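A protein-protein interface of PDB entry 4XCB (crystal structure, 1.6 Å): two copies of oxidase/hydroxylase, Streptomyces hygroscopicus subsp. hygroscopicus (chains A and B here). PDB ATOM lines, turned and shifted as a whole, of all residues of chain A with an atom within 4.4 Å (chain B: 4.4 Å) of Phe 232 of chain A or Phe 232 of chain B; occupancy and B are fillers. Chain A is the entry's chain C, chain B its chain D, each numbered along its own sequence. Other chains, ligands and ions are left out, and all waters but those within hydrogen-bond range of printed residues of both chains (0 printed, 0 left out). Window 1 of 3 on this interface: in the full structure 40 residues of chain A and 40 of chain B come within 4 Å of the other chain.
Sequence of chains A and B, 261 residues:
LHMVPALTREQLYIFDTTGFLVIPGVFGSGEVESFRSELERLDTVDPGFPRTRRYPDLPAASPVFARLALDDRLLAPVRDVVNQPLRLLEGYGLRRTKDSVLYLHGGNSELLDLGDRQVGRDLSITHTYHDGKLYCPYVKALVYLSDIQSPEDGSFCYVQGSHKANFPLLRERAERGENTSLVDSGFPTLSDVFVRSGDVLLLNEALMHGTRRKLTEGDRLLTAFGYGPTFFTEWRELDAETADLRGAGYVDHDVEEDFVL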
ATOM      1  N   ARG A  87      24.270 -21.526  21.233  1.00  0.00           N
ATOM      2  CA  ARG A  87      24.030 -20.151  20.814  1.00  0.00           C
ATOM      3  C   ARG A  87      25.198 -19.278  21.257  1.00  0.00           C
ATOM      4  O   ARG A  87      25.811 -19.540  22.289  1.00  0.00           O
ATOM      5  CB  ARG A  87      22.726 -19.622  21.407  1.00  0.00           C
ATOM      6  CG  ARG A  87      22.168 -18.419  20.697  1.00  0.00           C
ATOM      7  CD  ARG A  87      21.002 -17.794  21.455  1.00  0.00           C
ATOM      8  NE  ARG A  87      20.564 -16.571  20.793  1.00  0.00           N
ATOM      9  CZ  ARG A  87      19.511 -15.843  21.150  1.00  0.00           C
ATOM     10  NH1 ARG A  87      18.748 -16.201  22.176  1.00  0.00           N
ATOM     11  NH2 ARG A  87      19.212 -14.748  20.461  1.00  0.00           N
ATOM     12  N   LEU A  89      26.119 -16.030  23.008  1.00  0.00           N
ATOM     13  CA  LEU A  89      25.357 -15.190  23.922  1.00  0.00           C
ATOM     14  C   LEU A  89      25.940 -13.785  24.035  1.00  0.00           C
ATOM     15  O   LEU A  89      25.229 -12.817  24.332  1.00  0.00           O
ATOM     16  CB  LEU A  89      25.298 -15.847  25.302  1.00  0.00           C
ATOM     17  CG  LEU A  89      24.662 -17.236  25.270  1.00  0.00           C
ATOM     18  CD1 LEU A  89      24.599 -17.815  26.674  1.00  0.00           C
ATOM     19  CD2 LEU A  89      23.289 -17.167  24.633  1.00  0.00           C
ATOM     20  N   LEU A 123      20.276 -20.375  37.841  1.00  0.00           N
ATOM     21  CA  LEU A 123      20.123 -21.456  36.872  1.00  0.00           C
ATOM     22  C   LEU A 123      20.875 -21.202  35.583  1.00  0.00           C
ATOM     23  O   LEU A 123      21.096 -22.121  34.807  1.00  0.00           O
ATOM     24  CB  LEU A 123      18.639 -21.708  36.581  1.00  0.00           C
ATOM     25  CG  LEU A 123      17.942 -22.309  37.806  1.00  0.00           C
ATOM     26  CD1 LEU A 123      16.505 -22.686  37.542  1.00  0.00           C
ATOM     27  CD2 LEU A 123      18.714 -23.535  38.297  1.00  0.00           C
ATOM     28  N   SER A 124      21.331 -19.964  35.372  1.00  0.00           N
ATOM     29  CA  SER A 124      22.084 -19.657  34.175  1.00  0.00           C
ATOM     30  C   SER A 124      23.477 -20.263  34.227  1.00  0.00           C
ATOM     31  O   SER A 124      24.107 -20.475  33.202  1.00  0.00           O
ATOM     32  CB  SER A 124      22.183 -18.139  33.963  1.00  0.00           C
ATOM     33  OG  SER A 124      23.026 -17.532  34.928  1.00  0.00           O
ATOM     34  N   PRO A 137      25.687 -24.749  31.288  1.00  0.00           N
ATOM     35  CA  PRO A 137      24.851 -23.883  30.444  1.00  0.00           C
ATOM     36  C   PRO A 137      25.532 -22.585  30.016  1.00  0.00           C
ATOM     37  O   PRO A 137      25.137 -22.030  28.991  1.00  0.00           O
ATOM     38  CB  PRO A 137      23.650 -23.574  31.335  1.00  0.00           C
ATOM     39  CG  PRO A 137      24.179 -23.702  32.729  1.00  0.00           C
ATOM     40  CD  PRO A 137      25.255 -24.753  32.696  1.00  0.00           C
ATOM     41  N   PRO A 229      23.069 -22.709  25.656  1.00  0.00           N
ATOM     42  CA  PRO A 229      22.025 -23.364  24.866  1.00  0.00           C
ATOM     43  C   PRO A 229      21.255 -22.376  23.987  1.00  0.00           C
ATOM     44  O   PRO A 229      21.264 -21.186  24.255  1.00  0.00           O
ATOM     45  CB  PRO A 229      21.105 -23.958  25.932  1.00  0.00           C
ATOM     46  CG  PRO A 229      21.935 -24.032  27.189  1.00  0.00           C
ATOM     47  CD  PRO A 229      22.858 -22.851  27.102  1.00  0.00           C
ATOM     48  N   THR A 230      20.562 -22.889  22.980  1.00  0.00           N
ATOM     49  CA  THR A 230      19.783 -22.060  22.067  1.00  0.00           C
ATOM     50  C   THR A 230      18.613 -21.330  22.740  1.00  0.00           C
ATOM     51  O   THR A 230      18.104 -20.348  22.202  1.00  0.00           O
ATOM     52  CB  THR A 230      19.234 -22.899  20.907  1.00  0.00           C
ATOM     53  OG1 THR A 230      18.496 -24.012  21.436  1.00  0.00           O
ATOM     54  CG2 THR A 230      20.369 -23.431  20.043  1.00  0.00           C
ATOM     55  N   PHE A 231      18.183 -21.800  23.909  1.00  0.00           N
ATOM     56  CA  PHE A 231      17.052 -21.185  24.597  1.00  0.00           C
ATOM     57  C   PHE A 231      17.449 -20.108  25.594  1.00  0.00           C
ATOM     58  O   PHE A 231      16.595 -19.535  26.267  1.00  0.00           O
ATOM     59  CB  PHE A 231      16.216 -22.251  25.321  1.00  0.00           C
ATOM     60  CG  PHE A 231      17.031 -23.241  26.113  1.00  0.00           C
ATOM     61  CD1 PHE A 231      17.419 -24.446  25.541  1.00  0.00           C
ATOM     62  CD2 PHE A 231      17.385 -22.981  27.426  1.00  0.00           C
ATOM     63  CE1 PHE A 231      18.147 -25.375  26.269  1.00  0.00           C
ATOM     64  CE2 PHE A 231      18.130 -23.911  28.157  1.00  0.00           C
ATOM     65  CZ  PHE A 231      18.512 -25.094  27.574  1.00  0.00           C
ATOM     66  N   PHE A 232      18.748 -19.850  25.707  1.00  0.00           N
ATOM     67  CA  PHE A 232      19.236 -18.727  26.500  1.00  0.00           C
ATOM     68  C   PHE A 232      19.168 -17.450  25.667  1.00  0.00           C
ATOM     69  O   PHE A 232      19.445 -17.491  24.477  1.00  0.00           O
ATOM     70  CB  PHE A 232      20.680 -18.956  26.952  1.00  0.00           C
ATOM     71  CG  PHE A 232      20.816 -19.686  28.269  1.00  0.00           C
ATOM     72  CD1 PHE A 232      19.786 -20.464  28.782  1.00  0.00           C
ATOM     73  CD2 PHE A 232      21.998 -19.602  28.980  1.00  0.00           C
ATOM     74  CE1 PHE A 232      19.946 -21.126  29.992  1.00  0.00           C
ATOM     75  CE2 PHE A 232      22.153 -20.256  30.178  1.00  0.00           C
ATOM     76  CZ  PHE A 232      21.123 -21.026  30.686  1.00  0.00           C
ATOM     77  N   THR A 233      18.790 -16.342  26.288  1.00  0.00           N
ATOM     78  CA  THR A 233      18.883 -15.029  25.606  1.00  0.00           C
ATOM     79  C   THR A 233      20.312 -14.506  25.590  1.00  0.00           C
ATOM     80  O   THR A 233      21.102 -14.785  26.493  1.00  0.00           O
ATOM     81  CB  THR A 233      17.995 -13.969  26.265  1.00  0.00           C
ATOM     82  OG1 THR A 233      18.418 -13.745  27.616  1.00  0.00           O
ATOM     83  CG2 THR A 233      16.529 -14.391  26.246  1.00  0.00           C
ATOM     84  N   GLU A 234      20.634 -13.722  24.562  1.00  0.00           N
ATOM     85  CA  GLU A 234      21.948 -13.097  24.465  1.00  0.00           C
ATOM     86  C   GLU A 234      22.188 -12.270  25.710  1.00  0.00           C
ATOM     87  O   GLU A 234      21.236 -11.774  26.318  1.00  0.00           O
ATOM     88  CB  GLU A 234      22.034 -12.237  23.207  1.00  0.00           C
ATOM     89  CG  GLU A 234      21.718 -12.999  21.938  1.00  0.00           C
ATOM     90  CD  GLU A 234      21.751 -12.121  20.697  1.00  0.00           C
ATOM     91  OE1 GLU A 234      21.503 -10.902  20.817  1.00  0.00           O
ATOM     92  OE2 GLU A 234      22.033 -12.656  19.604  1.00  0.00           O
ATOM     93  N   TYR A 250      20.033 -11.194  32.407  1.00  0.00           N
ATOM     94  CA  TYR A 250      20.652 -11.990  33.453  1.00  0.00           C
ATOM     95  C   TYR A 250      20.764 -11.163  34.730  1.00  0.00           C
ATOM     96  O   TYR A 250      21.287 -10.042  34.715  1.00  0.00           O
ATOM     97  CB  TYR A 250      22.018 -12.488  33.005  1.00  0.00           C
ATOM     98  CG  TYR A 250      21.990 -13.430  31.821  1.00  0.00           C
ATOM     99  CD1 TYR A 250      21.675 -12.979  30.540  1.00  0.00           C
ATOM    100  CD2 TYR A 250      22.294 -14.775  31.981  1.00  0.00           C
ATOM    101  CE1 TYR A 250      21.658 -13.843  29.458  1.00  0.00           C
ATOM    102  CE2 TYR A 250      22.285 -15.643  30.911  1.00  0.00           C
ATOM    103  CZ  TYR A 250      21.952 -15.183  29.654  1.00  0.00           C
ATOM    104  OH  TYR A 250      21.953 -16.065  28.598  1.00  0.00           O
ATOM    105  N   ARG B  87      10.013 -14.712  33.842  1.00  0.00           N
ATOM    106  CA  ARG B  87       9.654 -14.207  32.522  1.00  0.00           C
ATOM    107  C   ARG B  87       8.535 -15.072  31.937  1.00  0.00           C
ATOM    108  O   ARG B  87       8.377 -16.227  32.325  1.00  0.00           O
ATOM    109  CB  ARG B  87      10.869 -14.203  31.590  1.00  0.00           C
ATOM    110  CG  ARG B  87      10.658 -13.427  30.305  1.00  0.00           C
ATOM    111  CD  ARG B  87      11.747 -13.646  29.255  1.00  0.00           C
ATOM    112  NE  ARG B  87      11.418 -12.881  28.051  1.00  0.00           N
ATOM    113  CZ  ARG B  87      12.122 -12.871  26.923  1.00  0.00           C
ATOM    114  NH1 ARG B  87      13.234 -13.580  26.808  1.00  0.00           N
ATOM    115  NH2 ARG B  87      11.711 -12.133  25.899  1.00  0.00           N
ATOM    116  N   LEU B  89       7.324 -17.160  28.836  1.00  0.00           N
ATOM    117  CA  LEU B  89       7.960 -17.803  27.700  1.00  0.00           C
ATOM    118  C   LEU B  89       6.959 -18.105  26.591  1.00  0.00           C
ATOM    119  O   LEU B  89       7.340 -18.197  25.420  1.00  0.00           O
ATOM    120  CB  LEU B  89       8.664 -19.089  28.141  1.00  0.00           C
ATOM    121  CG  LEU B  89       9.695 -18.898  29.249  1.00  0.00           C
ATOM    122  CD1 LEU B  89      10.494 -20.189  29.432  1.00  0.00           C
ATOM    123  CD2 LEU B  89      10.622 -17.728  28.945  1.00  0.00           C
ATOM    124  N   LEU B 123      18.870 -29.005  29.174  1.00  0.00           N
ATOM    125  CA  LEU B 123      19.057 -28.035  30.248  1.00  0.00           C
ATOM    126  C   LEU B 123      17.878 -27.075  30.429  1.00  0.00           C
ATOM    127  O   LEU B 123      17.767 -26.403  31.449  1.00  0.00           O
ATOM    128  CB  LEU B 123      20.355 -27.250  30.035  1.00  0.00           C
ATOM    129  CG  LEU B 123      21.620 -28.092  30.256  1.00  0.00           C
ATOM    130  CD1 LEU B 123      22.845 -27.210  30.300  1.00  0.00           C
ATOM    131  CD2 LEU B 123      21.558 -28.929  31.532  1.00  0.00           C
ATOM    132  N   SER B 124      16.970 -27.021  29.458  1.00  0.00           N
ATOM    133  CA  SER B 124      15.800 -26.168  29.595  1.00  0.00           C
ATOM    134  C   SER B 124      14.778 -26.700  30.593  1.00  0.00           C
ATOM    135  O   SER B 124      13.919 -25.958  31.065  1.00  0.00           O
ATOM    136  CB  SER B 124      15.124 -25.964  28.230  1.00  0.00           C
ATOM    137  OG  SER B 124      14.520 -27.152  27.743  1.00  0.00           O
ATOM    138  N   PRO B 137      13.458 -24.693  35.923  1.00  0.00           N
ATOM    139  CA  PRO B 137      13.619 -23.634  34.918  1.00  0.00           C
ATOM    140  C   PRO B 137      12.424 -23.495  33.975  1.00  0.00           C
ATOM    141  O   PRO B 137      12.216 -22.415  33.441  1.00  0.00           O
ATOM    142  CB  PRO B 137      14.860 -24.077  34.149  1.00  0.00           C
ATOM    143  CG  PRO B 137      14.885 -25.545  34.304  1.00  0.00           C
ATOM    144  CD  PRO B 137      14.413 -25.791  35.700  1.00  0.00           C
ATOM    145  N   PRO B 229      13.139 -18.523  33.784  1.00  0.00           N
ATOM    146  CA  PRO B 229      13.976 -17.423  34.265  1.00  0.00           C
ATOM    147  C   PRO B 229      14.087 -16.320  33.215  1.00  0.00           C
ATOM    148  O   PRO B 229      13.758 -16.551  32.053  1.00  0.00           O
ATOM    149  CB  PRO B 229      15.321 -18.102  34.525  1.00  0.00           C
ATOM    150  CG  PRO B 229      15.005 -19.566  34.651  1.00  0.00           C
ATOM    151  CD  PRO B 229      13.887 -19.790  33.701  1.00  0.00           C
ATOM    152  N   THR B 230      14.558 -15.141  33.613  1.00  0.00           N
ATOM    153  CA  THR B 230      14.594 -14.017  32.682  1.00  0.00           C
ATOM    154  C   THR B 230      15.610 -14.200  31.553  1.00  0.00           C
ATOM    155  O   THR B 230      15.537 -13.516  30.527  1.00  0.00           O
ATOM    156  CB  THR B 230      14.890 -12.704  33.416  1.00  0.00           C
ATOM    157  OG1 THR B 230      16.052 -12.864  34.233  1.00  0.00           O
ATOM    158  CG2 THR B 230      13.724 -12.299  34.283  1.00  0.00           C
ATOM    159  N   PHE B 231      16.550 -15.119  31.716  1.00  0.00           N
ATOM    160  CA  PHE B 231      17.508 -15.392  30.658  1.00  0.00           C
ATOM    161  C   PHE B 231      17.050 -16.501  29.713  1.00  0.00           C
ATOM    162  O   PHE B 231      17.804 -16.911  28.830  1.00  0.00           O
ATOM    163  CB  PHE B 231      18.877 -15.736  31.255  1.00  0.00           C
ATOM    164  CG  PHE B 231      18.820 -16.786  32.321  1.00  0.00           C
ATOM    165  CD1 PHE B 231      18.572 -16.435  33.643  1.00  0.00           C
ATOM    166  CD2 PHE B 231      18.987 -18.117  31.997  1.00  0.00           C
ATOM    167  CE1 PHE B 231      18.520 -17.397  34.627  1.00  0.00           C
ATOM    168  CE2 PHE B 231      18.924 -19.085  32.976  1.00  0.00           C
ATOM    169  CZ  PHE B 231      18.680 -18.720  34.289  1.00  0.00           C
ATOM    170  N   PHE B 232      15.835 -17.014  29.904  1.00  0.00           N
ATOM    171  CA  PHE B 232      15.286 -17.922  28.904  1.00  0.00           C
ATOM    172  C   PHE B 232      14.654 -17.113  27.770  1.00  0.00           C
ATOM    173  O   PHE B 232      14.055 -16.065  28.011  1.00  0.00           O
ATOM    174  CB  PHE B 232      14.252 -18.890  29.507  1.00  0.00           C
ATOM    175  CG  PHE B 232      14.849 -20.172  30.046  1.00  0.00           C
ATOM    176  CD1 PHE B 232      16.196 -20.260  30.363  1.00  0.00           C
ATOM    177  CD2 PHE B 232      14.053 -21.292  30.216  1.00  0.00           C
ATOM    178  CE1 PHE B 232      16.731 -21.443  30.867  1.00  0.00           C
ATOM    179  CE2 PHE B 232      14.589 -22.480  30.721  1.00  0.00           C
ATOM    180  CZ  PHE B 232      15.923 -22.553  31.032  1.00  0.00           C
ATOM    181  N   THR B 233      14.791 -17.608  26.546  1.00  0.00           N
ATOM    182  CA  THR B 233      14.082 -17.022  25.408  1.00  0.00           C
ATOM    183  C   THR B 233      12.636 -17.479  25.377  1.00  0.00           C
ATOM    184  O   THR B 233      12.302 -18.543  25.903  1.00  0.00           O
ATOM    185  CB  THR B 233      14.725 -17.397  24.060  1.00  0.00           C
ATOM    186  OG1 THR B 233      14.449 -18.771  23.756  1.00  0.00           O
ATOM    187  CG2 THR B 233      16.219 -17.183  24.089  1.00  0.00           C
ATOM    188  N   GLU B 234      11.779 -16.676  24.755  1.00  0.00           N
ATOM    189  CA  GLU B 234      10.390 -17.070  24.537  1.00  0.00           C
ATOM    190  C   GLU B 234      10.365 -18.333  23.687  1.00  0.00           C
ATOM    191  O   GLU B 234      11.248 -18.535  22.841  1.00  0.00           O
ATOM    192  CB  GLU B 234       9.606 -15.933  23.867  1.00  0.00           C
ATOM    193  CG  GLU B 234       9.084 -14.878  24.841  1.00  0.00           C
ATOM    194  CD  GLU B 234       8.634 -13.610  24.128  1.00  0.00           C
ATOM    195  OE1 GLU B 234       8.440 -13.667  22.896  1.00  0.00           O
ATOM    196  OE2 GLU B 234       8.485 -12.560  24.790  1.00  0.00           O
ATOM    197  N   TYR B 250      14.134 -23.883  21.100  1.00  0.00           N
ATOM    198  CA  TYR B 250      14.180 -25.087  21.928  1.00  0.00           C
ATOM    199  C   TYR B 250      14.231 -26.330  21.058  1.00  0.00           C
ATOM    200  O   TYR B 250      13.371 -26.530  20.201  1.00  0.00           O
ATOM    201  CB  TYR B 250      12.966 -25.131  22.847  1.00  0.00           C
ATOM    202  CG  TYR B 250      12.932 -24.026  23.874  1.00  0.00           C
ATOM    203  CD1 TYR B 250      12.714 -22.702  23.495  1.00  0.00           C
ATOM    204  CD2 TYR B 250      13.121 -24.297  25.224  1.00  0.00           C
ATOM    205  CE1 TYR B 250      12.681 -21.689  24.426  1.00  0.00           C
ATOM    206  CE2 TYR B 250      13.081 -23.290  26.169  1.00  0.00           C
ATOM    207  CZ  TYR B 250      12.868 -21.981  25.763  1.00  0.00           C
ATOM    208  OH  TYR B 250      12.842 -20.960  26.688  1.00  0.00           O
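The backbone carbonyl oxygen (O) of Phe 231 of chain B lies within hydrogen-bond range of the backbone NH (N) of Thr 233 of chain A (2.8 Å). The backbone carbonyl oxygen (O) of Phe 231 of chain A lies within hydrogen-bond range of the backbone NH (N) of Thr 233 of chain B (2.7 Å).
Arg 87 of chain A touches Thr 233 of chain B, and with the chains exchanged Thr 233 of chain A touches Arg 87 of chain B. Phe 231 of chain B touches its own counterpart, Phe 231 of chain A. Phe 232 of chain A touches Thr 233 of chain B, and with the chains exchanged Thr 233 of chain A touches Phe 232 of chain B. Thr 233 of chain A touches its own counterpart, Thr 233 of chain B. Positions printed for both chains: 87, 89, 123, 124, 137, 229, 230, 231, 232, 233, 234 and 250.
The backbone carbonyl oxygen (O) of Thr 233 of chain A sits at hydrogen-bond distance from the side-chain hydroxyl (OH) of Tyr 250 of chain A (2.6 Å). The backbone carbonyl oxygen of Thr 233 of chain B sits at hydrogen-bond distance from the side-chain hydroxyl of Tyr 250 of chain B (2.6 Å). NH2 of Arg 87 of chain B is in salt-bridge range of OE2 of Glu 234 of chain B (3.4 Å). The guanidinium group (NH2) of Arg 87 of chain A is in salt-bridge range of the side-chain carboxylate (OE2) of Glu 234 of chain A. The guanidinium group of Arg 87 of chain B sits at hydrogen-bond distance from the backbone carbonyl oxygen of Phe 232 of chain B (2.9 Å). The guanidinium group of Arg 87 of chain A sits at hydrogen-bond distance from the backbone carbonyl oxygen of Phe 232 of chain A (2.7 Å).
Phe 232 of chain A touches three residues of chain B. Of chain A, only Phe 231, Phe 232 and Thr 233 come within 4 Å of Phe 232 of chain B. Printed residues of chain B within 4 Å of Phe 231 of chain A: Leu 123 (3.5 Å), Ser 124 (3.1 Å), Phe 231 (3.9 Å), Phe 232 (3.4 Å), Thr 233 (2.7 Å) and Tyr 250 (3.4 Å). Printed residues of chain B within 4 Å of Thr 233 of chain A: Arg 87, Phe 231, Phe 232 and Thr 233. Printed residues of chain B within 4 Å of Ser 124 of chain A: Phe 231. Thr 230 of chain B touches none of the printed residues of chain A. Pro 229 of chain A touches none of the printed residues of chain B. The nearest printed residue of chain B that does not touch Phe 232 of chain A is Leu 123 of chain B (5.9 Å).
Of the 12 printed residues of chain A, 8 touch a printed residue of chain B. Hydrophobic or aromatic side chains of chain A within 4 Å of the printed part of chain B: Leu 123, Pro 137, Phe 231, Phe 232 and Tyr 250. Printed residues of chain B that touch a printed residue of chain A: Arg 87, Leu 123, Ser 124, Pro 137, Phe 231, Phe 232, Thr 233 and Tyr 250. Hydrophobic or aromatic side chains of chain B within 4 Å of the printed part of chain A: Leu 123, Phe 231, Phe 232 and Tyr 250. Among the printed residues, 19 pairs touch across the chains.
Among the printed residues, merely in contact across the chains: Phe 231 of chain A with Ser 124 of chain B (3.1 Å), Ser 124 of chain A with Phe 231 of chain B (3.1 Å), Phe 232 of chain A with Thr 233 of chain B (3.3 Å), Phe 232 of chain A with Phe 231 of chain B (3.3 Å), Arg 87 of chain A with Thr 233 of chain B (3.3 Å), Phe 232 of chain A with Phe 232 of chain B (3.3 Å), Phe 231 of chain A with Phe 232 of chain B (3.4 Å), Phe 231 of chain A with Tyr 250 of chain B (3.4 Å), Tyr 250 of chain A with Phe 231 of chain B (3.4 Å), Thr 233 of chain A with Arg 87 of chain B (3.4 Å), Thr 233 of chain A with Phe 232 of chain B (3.5 Å), Thr 233 of chain A with Thr 233 of chain B (3.5 Å), Phe 231 of chain A with Leu 123 of chain B (3.5 Å), Leu 123 of chain A with Phe 231 of chain B (3.6 Å), Phe 231 of chain A with Phe 231 of chain B (3.9 Å), Pro 137 of chain A with Leu 123 of chain B (3.9 Å) and Leu 123 of chain A with Pro 137 of chain B (3.99 Å).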
